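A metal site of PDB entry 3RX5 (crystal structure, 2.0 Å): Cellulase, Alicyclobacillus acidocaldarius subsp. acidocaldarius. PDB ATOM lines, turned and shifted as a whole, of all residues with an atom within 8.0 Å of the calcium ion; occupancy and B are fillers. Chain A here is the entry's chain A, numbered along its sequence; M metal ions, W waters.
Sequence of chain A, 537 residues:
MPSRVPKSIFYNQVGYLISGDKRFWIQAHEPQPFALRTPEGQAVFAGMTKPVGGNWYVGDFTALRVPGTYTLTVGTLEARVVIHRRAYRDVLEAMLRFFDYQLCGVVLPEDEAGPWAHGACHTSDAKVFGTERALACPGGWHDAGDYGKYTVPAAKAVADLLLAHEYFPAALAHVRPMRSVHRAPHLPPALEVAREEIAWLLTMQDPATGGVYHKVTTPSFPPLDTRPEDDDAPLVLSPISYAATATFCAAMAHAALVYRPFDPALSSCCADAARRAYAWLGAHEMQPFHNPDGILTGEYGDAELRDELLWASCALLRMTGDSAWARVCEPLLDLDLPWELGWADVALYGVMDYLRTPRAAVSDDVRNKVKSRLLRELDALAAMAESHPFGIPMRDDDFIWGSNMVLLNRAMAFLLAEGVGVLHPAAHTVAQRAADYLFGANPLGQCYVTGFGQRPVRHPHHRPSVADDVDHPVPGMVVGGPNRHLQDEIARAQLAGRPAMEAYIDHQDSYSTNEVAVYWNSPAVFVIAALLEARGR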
ATOM      1  N   VAL A 152     -10.500 -18.367 -19.924  1.00  0.00           N
ATOM      2  CA  VAL A 152      -9.078 -18.524 -20.203  1.00  0.00           C
ATOM      3  C   VAL A 152      -8.556 -17.339 -21.023  1.00  0.00           C
ATOM      4  O   VAL A 152      -7.707 -16.621 -20.488  1.00  0.00           O
ATOM      5  CB  VAL A 152      -8.762 -19.955 -20.776  1.00  0.00           C
ATOM      6  CG1 VAL A 152      -7.369 -20.030 -21.387  1.00  0.00           C
ATOM      7  CG2 VAL A 152      -8.942 -21.009 -19.698  1.00  0.00           C
ATOM      8  N   ALA A 243      -8.073 -25.011 -15.990  1.00  0.00           N
ATOM      9  CA  ALA A 243      -7.446 -23.891 -16.711  1.00  0.00           C
ATOM     10  C   ALA A 243      -8.156 -22.582 -16.383  1.00  0.00           C
ATOM     11  O   ALA A 243      -7.486 -21.586 -16.119  1.00  0.00           O
ATOM     12  CB  ALA A 243      -7.495 -24.145 -18.210  1.00  0.00           C
ATOM     13  N   THR A 247      -6.325 -19.538 -14.437  1.00  0.00           N
ATOM     14  CA  THR A 247      -6.106 -18.250 -15.135  1.00  0.00           C
ATOM     15  C   THR A 247      -6.901 -17.119 -14.438  1.00  0.00           C
ATOM     16  O   THR A 247      -6.409 -16.011 -14.318  1.00  0.00           O
ATOM     17  CB  THR A 247      -6.406 -18.333 -16.642  1.00  0.00           C
ATOM     18  OG1 THR A 247      -7.745 -18.797 -16.815  1.00  0.00           O
ATOM     19  CG2 THR A 247      -5.431 -19.247 -17.386  1.00  0.00           C
ATOM     20  N   GLY A 301      -9.291 -25.399 -25.310  1.00  0.00           N
ATOM     21  CA  GLY A 301      -8.742 -26.571 -24.661  1.00  0.00           C
ATOM     22  C   GLY A 301      -7.242 -26.412 -24.522  1.00  0.00           C
ATOM     23  O   GLY A 301      -6.637 -25.550 -25.174  1.00  0.00           O
ATOM     24  N   ASP A 302      -6.622 -27.267 -23.706  1.00  0.00           N
ATOM     25  CA  ASP A 302      -5.179 -27.219 -23.438  1.00  0.00           C
ATOM     26  C   ASP A 302      -4.842 -28.414 -22.574  1.00  0.00           C
ATOM     27  O   ASP A 302      -5.426 -28.527 -21.512  1.00  0.00           O
ATOM     28  CB  ASP A 302      -4.864 -25.923 -22.635  1.00  0.00           C
ATOM     29  CG  ASP A 302      -3.404 -25.699 -22.288  1.00  0.00           C
ATOM     30  OD1 ASP A 302      -2.527 -26.268 -22.999  1.00  0.00           O
ATOM     31  OD2 ASP A 302      -3.135 -24.863 -21.399  1.00  0.00           O
ATOM     32  N   ALA A 303      -3.915 -29.290 -23.004  1.00  0.00           N
ATOM     33  CA  ALA A 303      -3.542 -30.487 -22.228  1.00  0.00           C
ATOM     34  C   ALA A 303      -2.535 -30.177 -21.142  1.00  0.00           C
ATOM     35  O   ALA A 303      -2.411 -30.958 -20.198  1.00  0.00           O
ATOM     36  CB  ALA A 303      -2.992 -31.567 -23.151  1.00  0.00           C
ATOM     37  N   GLU A 304      -1.799 -29.055 -21.264  1.00  0.00           N
ATOM     38  CA  GLU A 304      -0.742 -28.666 -20.327  1.00  0.00           C
ATOM     39  C   GLU A 304      -1.217 -27.591 -19.381  1.00  0.00           C
ATOM     40  O   GLU A 304      -1.463 -26.461 -19.801  1.00  0.00           O
ATOM     41  CB  GLU A 304       0.517 -28.204 -21.095  1.00  0.00           C
ATOM     42  CG  GLU A 304       1.660 -27.820 -20.163  1.00  0.00           C
ATOM     43  CD  GLU A 304       2.142 -28.916 -19.225  1.00  0.00           C
ATOM     44  OE1 GLU A 304       2.746 -29.898 -19.704  1.00  0.00           O
ATOM     45  OE2 GLU A 304       1.850 -28.815 -18.010  1.00  0.00           O
ATOM     46  N   LEU A 305      -1.320 -27.926 -18.078  1.00  0.00           N
ATOM     47  CA  LEU A 305      -1.856 -27.035 -17.084  1.00  0.00           C
ATOM     48  C   LEU A 305      -0.871 -26.574 -16.007  1.00  0.00           C
ATOM     49  O   LEU A 305      -1.271 -25.807 -15.142  1.00  0.00           O
ATOM     50  CB  LEU A 305      -3.156 -27.636 -16.474  1.00  0.00           C
ATOM     51  CG  LEU A 305      -4.261 -27.990 -17.527  1.00  0.00           C
ATOM     52  CD1 LEU A 305      -5.405 -28.800 -16.896  1.00  0.00           C
ATOM     53  CD2 LEU A 305      -4.821 -26.732 -18.220  1.00  0.00           C
ATOM     54  N   ARG A 306       0.408 -27.008 -16.079  1.00  0.00           N
ATOM     55  CA  ARG A 306       1.391 -26.582 -15.064  1.00  0.00           C
ATOM     56  C   ARG A 306       1.745 -25.126 -15.190  1.00  0.00           C
ATOM     57  O   ARG A 306       2.036 -24.477 -14.185  1.00  0.00           O
ATOM     58  CB  ARG A 306       2.644 -27.474 -15.034  1.00  0.00           C
ATOM     59  CG  ARG A 306       2.346 -28.869 -14.462  1.00  0.00           C
ATOM     60  CD  ARG A 306       3.443 -29.880 -14.713  1.00  0.00           C
ATOM     61  NE  ARG A 306       3.618 -30.110 -16.151  1.00  0.00           N
ATOM     62  CZ  ARG A 306       4.573 -30.877 -16.664  1.00  0.00           C
ATOM     63  NH1 ARG A 306       5.461 -31.471 -15.867  1.00  0.00           N
ATOM     64  NH2 ARG A 306       4.679 -31.033 -17.971  1.00  0.00           N
ATOM     65  N   ASP A 307       1.718 -24.592 -16.427  1.00  0.00           N
ATOM     66  CA  ASP A 307       2.015 -23.185 -16.682  1.00  0.00           C
ATOM     67  C   ASP A 307       0.945 -22.274 -16.062  1.00  0.00           C
ATOM     68  O   ASP A 307       1.292 -21.245 -15.487  1.00  0.00           O
ATOM     69  CB  ASP A 307       2.229 -22.937 -18.194  1.00  0.00           C
ATOM     70  CG  ASP A 307       1.105 -23.426 -19.064  1.00  0.00           C
ATOM     71  OD1 ASP A 307       0.855 -24.655 -19.081  1.00  0.00           O
ATOM     72  OD2 ASP A 307       0.446 -22.578 -19.699  1.00  0.00           O
ATOM     73  N   GLU A 308      -0.356 -22.706 -16.093  1.00  0.00           N
ATOM     74  CA  GLU A 308      -1.459 -21.978 -15.463  1.00  0.00           C
ATOM     75  C   GLU A 308      -1.251 -21.972 -13.940  1.00  0.00           C
ATOM     76  O   GLU A 308      -1.424 -20.921 -13.306  1.00  0.00           O
ATOM     77  CB  GLU A 308      -2.826 -22.659 -15.809  1.00  0.00           C
ATOM     78  CG  GLU A 308      -3.342 -22.382 -17.218  1.00  0.00           C
ATOM     79  CD  GLU A 308      -2.592 -23.006 -18.377  1.00  0.00           C
ATOM     80  OE1 GLU A 308      -1.771 -23.931 -18.168  1.00  0.00           O
ATOM     81  OE2 GLU A 308      -2.811 -22.535 -19.511  1.00  0.00           O
ATOM     82  N   LEU A 309      -0.910 -23.142 -13.342  1.00  0.00           N
ATOM     83  CA  LEU A 309      -0.650 -23.228 -11.905  1.00  0.00           C
ATOM     84  C   LEU A 309       0.565 -22.323 -11.555  1.00  0.00           C
ATOM     85  O   LEU A 309       0.568 -21.652 -10.539  1.00  0.00           O
ATOM     86  CB  LEU A 309      -0.357 -24.669 -11.489  1.00  0.00           C
ATOM     87  CG  LEU A 309      -0.001 -24.902  -9.996  1.00  0.00           C
ATOM     88  CD1 LEU A 309      -1.162 -24.482  -9.044  1.00  0.00           C
ATOM     89  CD2 LEU A 309       0.372 -26.341  -9.752  1.00  0.00           C
ATOM     90  N   LEU A 337       8.772 -25.815 -19.517  1.00  0.00           N
ATOM     91  CA  LEU A 337       7.575 -25.232 -20.116  1.00  0.00           C
ATOM     92  C   LEU A 337       7.985 -24.065 -21.057  1.00  0.00           C
ATOM     93  O   LEU A 337       8.930 -23.327 -20.739  1.00  0.00           O
ATOM     94  CB  LEU A 337       6.655 -24.692 -19.002  1.00  0.00           C
ATOM     95  CG  LEU A 337       5.945 -25.723 -18.149  1.00  0.00           C
ATOM     96  CD1 LEU A 337       5.340 -25.091 -16.898  1.00  0.00           C
ATOM     97  CD2 LEU A 337       4.871 -26.449 -18.942  1.00  0.00           C
ATOM     98  N   PRO A 338       7.309 -23.864 -22.213  1.00  0.00           N
ATOM     99  CA  PRO A 338       7.637 -22.683 -23.042  1.00  0.00           C
ATOM    100  C   PRO A 338       7.239 -21.428 -22.245  1.00  0.00           C
ATOM    101  O   PRO A 338       6.252 -21.445 -21.502  1.00  0.00           O
ATOM    102  CB  PRO A 338       6.761 -22.859 -24.288  1.00  0.00           C
ATOM    103  CG  PRO A 338       5.670 -23.776 -23.883  1.00  0.00           C
ATOM    104  CD  PRO A 338       6.174 -24.634 -22.766  1.00  0.00           C
ATOM    105  N   GLY A 342       0.568 -16.638 -23.508  1.00  0.00           N
ATOM    106  CA  GLY A 342      -0.762 -17.163 -23.787  1.00  0.00           C
ATOM    107  C   GLY A 342      -1.210 -17.244 -25.229  1.00  0.00           C
ATOM    108  O   GLY A 342      -0.405 -17.040 -26.120  1.00  0.00           O
ATOM    109  N   TRP A 343      -2.499 -17.543 -25.487  1.00  0.00           N
ATOM    110  CA  TRP A 343      -3.538 -17.781 -24.473  1.00  0.00           C
ATOM    111  C   TRP A 343      -3.403 -19.119 -23.728  1.00  0.00           C
ATOM    112  O   TRP A 343      -3.855 -19.234 -22.587  1.00  0.00           O
ATOM    113  CB  TRP A 343      -4.945 -17.691 -25.110  1.00  0.00           C
ATOM    114  CG  TRP A 343      -5.194 -18.688 -26.203  1.00  0.00           C
ATOM    115  CD1 TRP A 343      -5.048 -18.470 -27.547  1.00  0.00           C
ATOM    116  CD2 TRP A 343      -5.633 -20.059 -26.063  1.00  0.00           C
ATOM    117  NE1 TRP A 343      -5.388 -19.612 -28.254  1.00  0.00           N
ATOM    118  CE2 TRP A 343      -5.802 -20.584 -27.359  1.00  0.00           C
ATOM    119  CE3 TRP A 343      -6.011 -20.863 -24.952  1.00  0.00           C
ATOM    120  CZ2 TRP A 343      -6.209 -21.911 -27.590  1.00  0.00           C
ATOM    121  CZ3 TRP A 343      -6.389 -22.193 -25.188  1.00  0.00           C
ATOM    122  CH2 TRP A 343      -6.453 -22.709 -26.493  1.00  0.00           C
ATOM    123  N   ALA A 344      -2.798 -20.138 -24.372  1.00  0.00           N
ATOM    124  CA  ALA A 344      -2.659 -21.496 -23.830  1.00  0.00           C
ATOM    125  C   ALA A 344      -1.381 -21.707 -22.997  1.00  0.00           C
ATOM    126  O   ALA A 344      -1.408 -22.408 -22.000  1.00  0.00           O
ATOM    127  CB  ALA A 344      -2.755 -22.531 -24.965  1.00  0.00           C
ATOM    128  N   ASP A 345      -0.272 -21.123 -23.429  1.00  0.00           N
ATOM    129  CA  ASP A 345       1.012 -21.265 -22.746  1.00  0.00           C
ATOM    130  C   ASP A 345       1.284 -19.925 -22.130  1.00  0.00           C
ATOM    131  O   ASP A 345       1.619 -18.981 -22.837  1.00  0.00           O
ATOM    132  CB  ASP A 345       2.092 -21.668 -23.763  1.00  0.00           C
ATOM    133  CG  ASP A 345       1.700 -22.928 -24.509  1.00  0.00           C
ATOM    134  OD1 ASP A 345       1.293 -22.801 -25.692  1.00  0.00           O
ATOM    135  OD2 ASP A 345       1.627 -24.013 -23.878  1.00  0.00           O
ATOM    136  N   VAL A 346       1.083 -19.836 -20.816  1.00  0.00           N
ATOM    137  CA  VAL A 346       1.104 -18.598 -20.034  1.00  0.00           C
ATOM    138  C   VAL A 346       2.257 -18.447 -19.032  1.00  0.00           C
ATOM    139  O   VAL A 346       2.231 -17.481 -18.263  1.00  0.00           O
ATOM    140  CB  VAL A 346      -0.281 -18.410 -19.299  1.00  0.00           C
ATOM    141  CG1 VAL A 346      -1.433 -18.264 -20.290  1.00  0.00           C
ATOM    142  CG2 VAL A 346      -0.566 -19.555 -18.316  1.00  0.00           C
ATOM    143  N   ALA A 347       3.229 -19.388 -19.006  1.00  0.00           N
ATOM    144  CA  ALA A 347       4.331 -19.380 -18.029  1.00  0.00           C
ATOM    145  C   ALA A 347       5.042 -18.015 -17.896  1.00  0.00           C
ATOM    146  O   ALA A 347       5.394 -17.650 -16.781  1.00  0.00           O
ATOM    147  CB  ALA A 347       5.349 -20.476 -18.348  1.00  0.00           C
HETATM  148 CA    CA M   1      -1.216 -24.156 -20.442  1.00  0.00          CA
HETATM  149  O   HOH W   1      -0.167 -25.180 -22.269  1.00  0.00           O
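N of Val 346 sits close to OD2 of Asp 307 (3.0 Å).
The guanidinium group (NH2) of Arg 306 is in salt-bridge range of the side-chain carboxylate (OE1) of Glu 304.
Along chain A the residues within 4 Å of the calcium ion span positions 302 to 344.
The calcium ion is bound by the side-chain carboxylate (OD2) of Asp 302 (2.3 Å), water W1 (2.3 Å), the backbone carbonyl oxygen (O) of Ala 344 (2.3 Å), the side-chain carboxylate (OE1) of Glu 308 (2.4 Å), the backbone carbonyl oxygen (O) of Glu 304 (2.4 Å), the side-chain carboxylate (OD2) of Asp 307 (2.4 Å), the side-chain carboxylate (OE2) of Glu 308 (2.5 Å) and the side-chain carboxylate (OD1) of Asp 307 (2.5 Å).
The calcium ion has eight donor atoms within binding distance.
Water W1 lies within hydrogen-bond range of the side-chain carboxylate of Asp 345 (2.7 Å) and the side-chain carboxylate of Asp 302 (2.7 Å).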
